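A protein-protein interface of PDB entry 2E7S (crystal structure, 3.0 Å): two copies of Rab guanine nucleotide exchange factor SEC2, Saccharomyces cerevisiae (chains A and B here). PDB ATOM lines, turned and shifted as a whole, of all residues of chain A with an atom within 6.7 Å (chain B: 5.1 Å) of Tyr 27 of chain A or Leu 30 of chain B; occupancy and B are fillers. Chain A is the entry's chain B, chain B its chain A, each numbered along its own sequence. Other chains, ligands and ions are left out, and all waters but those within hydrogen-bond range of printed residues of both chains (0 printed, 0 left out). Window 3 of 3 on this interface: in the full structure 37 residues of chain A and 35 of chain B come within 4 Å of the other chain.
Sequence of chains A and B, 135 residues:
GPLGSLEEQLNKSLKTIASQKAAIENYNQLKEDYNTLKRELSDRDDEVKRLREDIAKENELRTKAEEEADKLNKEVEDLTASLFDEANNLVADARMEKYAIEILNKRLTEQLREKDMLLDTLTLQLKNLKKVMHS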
ATOM      1  N   ALA A  22      15.804 -13.071  -8.766  1.00  0.00           N
ATOM      2  CA  ALA A  22      15.266 -13.611  -9.994  1.00  0.00           C
ATOM      3  C   ALA A  22      14.802 -15.044  -9.773  1.00  0.00           C
ATOM      4  O   ALA A  22      14.263 -15.666 -10.679  1.00  0.00           O
ATOM      5  CB  ALA A  22      16.306 -13.552 -11.099  1.00  0.00           C
ATOM      6  N   ALA A  23      14.989 -15.570  -8.567  1.00  0.00           N
ATOM      7  CA  ALA A  23      14.557 -16.933  -8.276  1.00  0.00           C
ATOM      8  C   ALA A  23      13.056 -16.970  -8.114  1.00  0.00           C
ATOM      9  O   ALA A  23      12.405 -17.928  -8.504  1.00  0.00           O
ATOM     10  CB  ALA A  23      15.214 -17.422  -7.033  1.00  0.00           C
ATOM     11  N   ILE A  24      12.518 -15.929  -7.502  1.00  0.00           N
ATOM     12  CA  ILE A  24      11.080 -15.805  -7.330  1.00  0.00           C
ATOM     13  C   ILE A  24      10.568 -15.094  -8.574  1.00  0.00           C
ATOM     14  O   ILE A  24       9.707 -15.587  -9.280  1.00  0.00           O
ATOM     15  CB  ILE A  24      10.712 -14.927  -6.115  1.00  0.00           C
ATOM     16  CG1 ILE A  24      10.754 -15.747  -4.842  1.00  0.00           C
ATOM     17  CG2 ILE A  24       9.322 -14.328  -6.275  1.00  0.00           C
ATOM     18  CD1 ILE A  24      10.260 -14.952  -3.640  1.00  0.00           C
ATOM     19  N   GLU A  25      11.117 -13.920  -8.826  1.00  0.00           N
ATOM     20  CA  GLU A  25      10.729 -13.121  -9.964  1.00  0.00           C
ATOM     21  C   GLU A  25      10.370 -14.014 -11.130  1.00  0.00           C
ATOM     22  O   GLU A  25       9.386 -13.770 -11.801  1.00  0.00           O
ATOM     23  CB  GLU A  25      11.869 -12.177 -10.359  1.00  0.00           C
ATOM     24  CG  GLU A  25      11.431 -10.952 -11.162  1.00  0.00           C
ATOM     25  CD  GLU A  25      12.600 -10.025 -11.529  1.00  0.00           C
ATOM     26  OE1 GLU A  25      13.430  -9.731 -10.636  1.00  0.00           O
ATOM     27  OE2 GLU A  25      12.683  -9.577 -12.705  1.00  0.00           O
ATOM     28  N   ASN A  26      11.152 -15.060 -11.366  1.00  0.00           N
ATOM     29  CA  ASN A  26      10.877 -15.955 -12.483  1.00  0.00           C
ATOM     30  C   ASN A  26       9.737 -16.912 -12.206  1.00  0.00           C
ATOM     31  O   ASN A  26       8.878 -17.107 -13.062  1.00  0.00           O
ATOM     32  CB  ASN A  26      12.125 -16.743 -12.854  1.00  0.00           C
ATOM     33  CG  ASN A  26      13.217 -15.863 -13.437  1.00  0.00           C
ATOM     34  OD1 ASN A  26      14.262 -16.360 -13.869  1.00  0.00           O
ATOM     35  ND2 ASN A  26      12.987 -14.550 -13.455  1.00  0.00           N
ATOM     36  N   TYR A  27       9.730 -17.513 -11.020  1.00  0.00           N
ATOM     37  CA  TYR A  27       8.666 -18.434 -10.646  1.00  0.00           C
ATOM     38  C   TYR A  27       7.323 -17.756 -10.893  1.00  0.00           C
ATOM     39  O   TYR A  27       6.399 -18.377 -11.411  1.00  0.00           O
ATOM     40  CB  TYR A  27       8.763 -18.809  -9.182  1.00  0.00           C
ATOM     41  CG  TYR A  27       7.634 -19.687  -8.719  1.00  0.00           C
ATOM     42  CD1 TYR A  27       7.681 -21.065  -8.900  1.00  0.00           C
ATOM     43  CD2 TYR A  27       6.532 -19.150  -8.053  1.00  0.00           C
ATOM     44  CE1 TYR A  27       6.657 -21.895  -8.413  1.00  0.00           C
ATOM     45  CE2 TYR A  27       5.505 -19.972  -7.567  1.00  0.00           C
ATOM     46  CZ  TYR A  27       5.575 -21.339  -7.743  1.00  0.00           C
ATOM     47  OH  TYR A  27       4.584 -22.145  -7.223  1.00  0.00           O
ATOM     48  N   ASN A  28       7.203 -16.488 -10.519  1.00  0.00           N
ATOM     49  CA  ASN A  28       5.964 -15.766 -10.757  1.00  0.00           C
ATOM     50  C   ASN A  28       5.837 -15.487 -12.263  1.00  0.00           C
ATOM     51  O   ASN A  28       4.751 -15.538 -12.828  1.00  0.00           O
ATOM     52  CB  ASN A  28       5.936 -14.464  -9.948  1.00  0.00           C
ATOM     53  CG  ASN A  28       5.748 -14.709  -8.472  1.00  0.00           C
ATOM     54  OD1 ASN A  28       4.913 -15.507  -8.078  1.00  0.00           O
ATOM     55  ND2 ASN A  28       6.512 -14.015  -7.650  1.00  0.00           N
ATOM     56  N   GLN A  29       6.960 -15.214 -12.913  1.00  0.00           N
ATOM     57  CA  GLN A  29       6.958 -14.943 -14.345  1.00  0.00           C
ATOM     58  C   GLN A  29       6.502 -16.196 -15.068  1.00  0.00           C
ATOM     59  O   GLN A  29       6.344 -16.199 -16.285  1.00  0.00           O
ATOM     60  CB  GLN A  29       8.365 -14.565 -14.842  1.00  0.00           C
ATOM     61  CG  GLN A  29       8.839 -13.113 -14.530  1.00  0.00           C
ATOM     62  CD  GLN A  29      10.215 -12.740 -15.164  1.00  0.00           C
ATOM     63  OE1 GLN A  29      10.352 -12.613 -16.388  1.00  0.00           O
ATOM     64  NE2 GLN A  29      11.223 -12.562 -14.318  1.00  0.00           N
ATOM     65  N   LEU A  30       6.320 -17.272 -14.318  1.00  0.00           N
ATOM     66  CA  LEU A  30       5.864 -18.514 -14.910  1.00  0.00           C
ATOM     67  C   LEU A  30       4.512 -18.904 -14.361  1.00  0.00           C
ATOM     68  O   LEU A  30       3.729 -19.503 -15.084  1.00  0.00           O
ATOM     69  CB  LEU A  30       6.840 -19.659 -14.666  1.00  0.00           C
ATOM     70  CG  LEU A  30       6.509 -20.959 -15.402  1.00  0.00           C
ATOM     71  CD1 LEU A  30       6.720 -20.753 -16.892  1.00  0.00           C
ATOM     72  CD2 LEU A  30       7.376 -22.080 -14.895  1.00  0.00           C
ATOM     73  N   LYS A  31       4.215 -18.580 -13.101  1.00  0.00           N
ATOM     74  CA  LYS A  31       2.902 -18.928 -12.558  1.00  0.00           C
ATOM     75  C   LYS A  31       1.847 -17.940 -13.010  1.00  0.00           C
ATOM     76  O   LYS A  31       0.655 -18.178 -12.892  1.00  0.00           O
ATOM     77  CB  LYS A  31       2.898 -18.994 -11.042  1.00  0.00           C
ATOM     78  CG  LYS A  31       1.592 -19.541 -10.535  1.00  0.00           C
ATOM     79  CD  LYS A  31       1.718 -20.124  -9.165  1.00  0.00           C
ATOM     80  CE  LYS A  31       0.390 -20.658  -8.692  1.00  0.00           C
ATOM     81  NZ  LYS A  31       0.515 -21.156  -7.300  1.00  0.00           N
ATOM     82  N   GLU A  32       2.294 -16.818 -13.534  1.00  0.00           N
ATOM     83  CA  GLU A  32       1.362 -15.849 -14.043  1.00  0.00           C
ATOM     84  C   GLU A  32       0.896 -16.380 -15.389  1.00  0.00           C
ATOM     85  O   GLU A  32      -0.273 -16.269 -15.730  1.00  0.00           O
ATOM     86  CB  GLU A  32       2.039 -14.503 -14.229  1.00  0.00           C
ATOM     87  CG  GLU A  32       1.054 -13.335 -14.435  1.00  0.00           C
ATOM     88  CD  GLU A  32       0.385 -12.852 -13.134  1.00  0.00           C
ATOM     89  OE1 GLU A  32      -0.126 -13.709 -12.369  1.00  0.00           O
ATOM     90  OE2 GLU A  32       0.366 -11.614 -12.889  1.00  0.00           O
ATOM     91  N   TYR A  34       1.100 -19.502 -16.128  1.00  0.00           N
ATOM     92  CA  TYR A  34       0.514 -20.793 -15.830  1.00  0.00           C
ATOM     93  C   TYR A  34      -0.945 -20.484 -15.641  1.00  0.00           C
ATOM     94  O   TYR A  34      -1.797 -21.096 -16.265  1.00  0.00           O
ATOM     95  CB  TYR A  34       1.067 -21.362 -14.535  1.00  0.00           C
ATOM     96  CG  TYR A  34       0.220 -22.448 -13.916  1.00  0.00           C
ATOM     97  CD1 TYR A  34       0.350 -23.767 -14.311  1.00  0.00           C
ATOM     98  CD2 TYR A  34      -0.709 -22.142 -12.917  1.00  0.00           C
ATOM     99  CE1 TYR A  34      -0.423 -24.757 -13.729  1.00  0.00           C
ATOM    100  CE2 TYR A  34      -1.485 -23.121 -12.324  1.00  0.00           C
ATOM    101  CZ  TYR A  34      -1.345 -24.431 -12.730  1.00  0.00           C
ATOM    102  OH  TYR A  34      -2.144 -25.404 -12.152  1.00  0.00           O
ATOM    103  N   GLU B  25      13.708 -27.091  -7.351  1.00  0.00           N
ATOM    104  CA  GLU B  25      12.618 -28.055  -7.295  1.00  0.00           C
ATOM    105  C   GLU B  25      11.296 -27.366  -7.636  1.00  0.00           C
ATOM    106  O   GLU B  25      10.526 -27.886  -8.441  1.00  0.00           O
ATOM    107  CB  GLU B  25      12.584 -28.709  -5.903  1.00  0.00           C
ATOM    108  CG  GLU B  25      11.698 -29.954  -5.776  1.00  0.00           C
ATOM    109  CD  GLU B  25      12.078 -30.864  -4.592  1.00  0.00           C
ATOM    110  OE1 GLU B  25      12.179 -30.377  -3.447  1.00  0.00           O
ATOM    111  OE2 GLU B  25      12.272 -32.082  -4.805  1.00  0.00           O
ATOM    112  N   ASN B  26      11.057 -26.188  -7.060  1.00  0.00           N
ATOM    113  CA  ASN B  26       9.835 -25.425  -7.326  1.00  0.00           C
ATOM    114  C   ASN B  26       9.615 -25.235  -8.821  1.00  0.00           C
ATOM    115  O   ASN B  26       8.645 -25.741  -9.386  1.00  0.00           O
ATOM    116  CB  ASN B  26       9.888 -24.027  -6.684  1.00  0.00           C
ATOM    117  CG  ASN B  26       9.760 -24.060  -5.176  1.00  0.00           C
ATOM    118  OD1 ASN B  26       9.197 -24.999  -4.617  1.00  0.00           O
ATOM    119  ND2 ASN B  26      10.266 -23.017  -4.509  1.00  0.00           N
ATOM    120  N   TYR B  27      10.517 -24.486  -9.445  1.00  0.00           N
ATOM    121  CA  TYR B  27      10.438 -24.202 -10.874  1.00  0.00           C
ATOM    122  C   TYR B  27      10.300 -25.485 -11.710  1.00  0.00           C
ATOM    123  O   TYR B  27       9.517 -25.518 -12.662  1.00  0.00           O
ATOM    124  CB  TYR B  27      11.690 -23.429 -11.333  1.00  0.00           C
ATOM    125  CG  TYR B  27      11.518 -22.479 -12.525  1.00  0.00           C
ATOM    126  CD1 TYR B  27      10.750 -21.317 -12.409  1.00  0.00           C
ATOM    127  CD2 TYR B  27      12.180 -22.706 -13.744  1.00  0.00           C
ATOM    128  CE1 TYR B  27      10.645 -20.397 -13.467  1.00  0.00           C
ATOM    129  CE2 TYR B  27      12.080 -21.790 -14.812  1.00  0.00           C
ATOM    130  CZ  TYR B  27      11.310 -20.633 -14.663  1.00  0.00           C
ATOM    131  OH  TYR B  27      11.207 -19.704 -15.687  1.00  0.00           O
ATOM    132  N   ASN B  28      11.039 -26.542 -11.367  1.00  0.00           N
ATOM    133  CA  ASN B  28      10.966 -27.765 -12.160  1.00  0.00           C
ATOM    134  C   ASN B  28       9.664 -28.518 -12.079  1.00  0.00           C
ATOM    135  O   ASN B  28       9.165 -28.973 -13.109  1.00  0.00           O
ATOM    136  CB  ASN B  28      12.128 -28.698 -11.853  1.00  0.00           C
ATOM    137  CG  ASN B  28      13.310 -28.418 -12.732  1.00  0.00           C
ATOM    138  OD1 ASN B  28      13.187 -28.425 -13.947  1.00  0.00           O
ATOM    139  ND2 ASN B  28      14.455 -28.154 -12.131  1.00  0.00           N
ATOM    140  N   GLN B  29       9.106 -28.662 -10.883  1.00  0.00           N
ATOM    141  CA  GLN B  29       7.837 -29.361 -10.788  1.00  0.00           C
ATOM    142  C   GLN B  29       6.707 -28.388 -11.157  1.00  0.00           C
ATOM    143  O   GLN B  29       5.541 -28.782 -11.194  1.00  0.00           O
ATOM    144  CB  GLN B  29       7.609 -29.952  -9.389  1.00  0.00           C
ATOM    145  CG  GLN B  29       6.453 -30.967  -9.344  1.00  0.00           C
ATOM    146  CD  GLN B  29       5.629 -30.911  -8.050  1.00  0.00           C
ATOM    147  OE1 GLN B  29       4.575 -31.551  -7.943  1.00  0.00           O
ATOM    148  NE2 GLN B  29       6.105 -30.142  -7.063  1.00  0.00           N
ATOM    149  N   LEU B  30       7.044 -27.124 -11.428  1.00  0.00           N
ATOM    150  CA  LEU B  30       6.034 -26.142 -11.837  1.00  0.00           C
ATOM    151  C   LEU B  30       6.019 -26.006 -13.363  1.00  0.00           C
ATOM    152  O   LEU B  30       4.952 -25.997 -13.982  1.00  0.00           O
ATOM    153  CB  LEU B  30       6.297 -24.762 -11.236  1.00  0.00           C
ATOM    154  CG  LEU B  30       5.356 -23.694 -11.819  1.00  0.00           C
ATOM    155  CD1 LEU B  30       4.011 -23.796 -11.126  1.00  0.00           C
ATOM    156  CD2 LEU B  30       5.940 -22.301 -11.641  1.00  0.00           C
ATOM    157  N   LYS B  31       7.201 -25.880 -13.965  1.00  0.00           N
ATOM    158  CA  LYS B  31       7.302 -25.763 -15.419  1.00  0.00           C
ATOM    159  C   LYS B  31       6.747 -27.091 -15.908  1.00  0.00           C
ATOM    160  O   LYS B  31       6.038 -27.163 -16.914  1.00  0.00           O
ATOM    161  CB  LYS B  31       8.768 -25.598 -15.853  1.00  0.00           C
ATOM    162  CG  LYS B  31       8.987 -25.192 -17.320  1.00  0.00           C
ATOM    163  CD  LYS B  31       8.722 -23.715 -17.570  1.00  0.00           C
ATOM    164  CE  LYS B  31       9.116 -23.303 -18.984  1.00  0.00           C
ATOM    165  NZ  LYS B  31       9.045 -21.819 -19.204  1.00  0.00           N
ATOM    166  N   GLU B  32       7.055 -28.143 -15.159  1.00  0.00           N
ATOM    167  CA  GLU B  32       6.586 -29.478 -15.487  1.00  0.00           C
ATOM    168  C   GLU B  32       5.047 -29.493 -15.517  1.00  0.00           C
ATOM    169  O   GLU B  32       4.445 -30.137 -16.377  1.00  0.00           O
ATOM    170  CB  GLU B  32       7.146 -30.480 -14.459  1.00  0.00           C
ATOM    171  CG  GLU B  32       6.880 -31.973 -14.747  1.00  0.00           C
ATOM    172  CD  GLU B  32       7.665 -32.934 -13.822  1.00  0.00           C
ATOM    173  OE1 GLU B  32       7.407 -34.158 -13.880  1.00  0.00           O
ATOM    174  OE2 GLU B  32       8.541 -32.480 -13.047  1.00  0.00           O
ATOM    175  N   ASP B  33       4.414 -28.770 -14.591  1.00  0.00           N
ATOM    176  CA  ASP B  33       2.952 -28.703 -14.520  1.00  0.00           C
ATOM    177  C   ASP B  33       2.421 -27.642 -15.482  1.00  0.00           C
ATOM    178  O   ASP B  33       1.218 -27.464 -15.613  1.00  0.00           O
ATOM    179  CB  ASP B  33       2.465 -28.395 -13.084  1.00  0.00           C
ATOM    180  CG  ASP B  33       2.777 -29.519 -12.085  1.00  0.00           C
ATOM    181  OD1 ASP B  33       2.667 -30.705 -12.451  1.00  0.00           O
ATOM    182  OD2 ASP B  33       3.112 -29.224 -10.919  1.00  0.00           O
ATOM    183  N   TYR B  34       3.319 -26.936 -16.152  1.00  0.00           N
ATOM    184  CA  TYR B  34       2.906 -25.922 -17.101  1.00  0.00           C
ATOM    185  C   TYR B  34       2.787 -26.549 -18.461  1.00  0.00           C
ATOM    186  O   TYR B  34       1.773 -26.409 -19.133  1.00  0.00           O
ATOM    187  CB  TYR B  34       3.933 -24.817 -17.203  1.00  0.00           C
ATOM    188  CG  TYR B  34       3.798 -23.987 -18.469  1.00  0.00           C
ATOM    189  CD1 TYR B  34       2.822 -23.008 -18.587  1.00  0.00           C
ATOM    190  CD2 TYR B  34       4.672 -24.169 -19.537  1.00  0.00           C
ATOM    191  CE1 TYR B  34       2.724 -22.228 -19.729  1.00  0.00           C
ATOM    192  CE2 TYR B  34       4.580 -23.399 -20.682  1.00  0.00           C
ATOM    193  CZ  TYR B  34       3.610 -22.428 -20.773  1.00  0.00           C
ATOM    194  OH  TYR B  34       3.551 -21.653 -21.909  1.00  0.00           O
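O of Gln 29 of chain B sits close to OD2 of Asp 33 of chain B. The backbone carbonyl oxygen (O) of Ala 22 of chain A lies close to the side-chain amide nitrogen (ND2) of Asn 26 of chain A. The side-chain amide nitrogen (ND2) of Asn 26 of chain A lies close to the side-chain amide nitrogen (NE2) of Gln 29 of chain A, 2.8 Å away.
Tyr 27 of chain B touches Asn 26 of chain A (CE1 to O, 3.8 Å). Tyr 27 of chain B touches Tyr 27 of chain A (CE1 to N, 3.9 Å). Leu 30 of chain B touches Tyr 27 of chain A (CD2 to CE1, 3.3 Å). Leu 30 of chain A touches Tyr 27 of chain B. Leu 30 of chain B touches Leu 30 of chain A (CD2 to CD2, 3.6 Å). Lys 31 of chain B touches Leu 30 of chain A. Tyr 34 of chain A touches Asp 33 of chain B.
Of the printed residues of chain B, Tyr 27 of chain A touches Tyr 27 and Leu 30. Of the printed residues of chain B, Leu 30 of chain A touches Tyr 27 (3.9 Å), Leu 30 (3.6 Å) and Lys 31 (3.4 Å). Printed residues of chain B within 4 Å of Tyr 34 of chain A: Asp 33. Leu 30 of chain B touches just these residues of chain A: Tyr 27 and Leu 30. Printed residues of chain A within 4 Å of Asp 33 of chain B: Tyr 34. The nearest residue of chain B that does not touch Tyr 27 of chain A is Asn 26 of chain B (4.2 Å). The nearest residue of chain A that does not touch Leu 30 of chain B is Lys 31 of chain A (4.4 Å).
Of the 10 printed residues of chain B, 4 touch a printed residue of chain A. Printed residues of chain B that touch a printed residue of chain A: Tyr 27, Leu 30, Lys 31 and Asp 33. Hydrophobic or aromatic side chains of chain B that line the printed part of chain A: Tyr 27 and Leu 30. Among the printed residues, 7 pairs touch across the chains. Among the printed residues, no Asp or Glu carboxylate lies within 4 Å of a Lys or Arg side-chain nitrogen of the other chain.
Asn 26 of chain A touches Tyr 27 of chain B, but with the chains exchanged Tyr 27 of chain A does not touch Asn 26 of chain B (4.2 Å). Tyr 27 of chain A touches its own counterpart, Tyr 27 of chain B. Tyr 27 of chain A touches Leu 30 of chain B, and with the chains exchanged Leu 30 of chain A touches Tyr 27 of chain B. Leu 30 of chain A touches Lys 31 of chain B, but with the chains exchanged Lys 31 of chain A does not touch Leu 30 of chain B (4.4 Å). 9 positions are printed for both chains. Of the 7 pairs that touch across the chains among the printed residues, 4 have their exchanged pair printed and touching as well.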
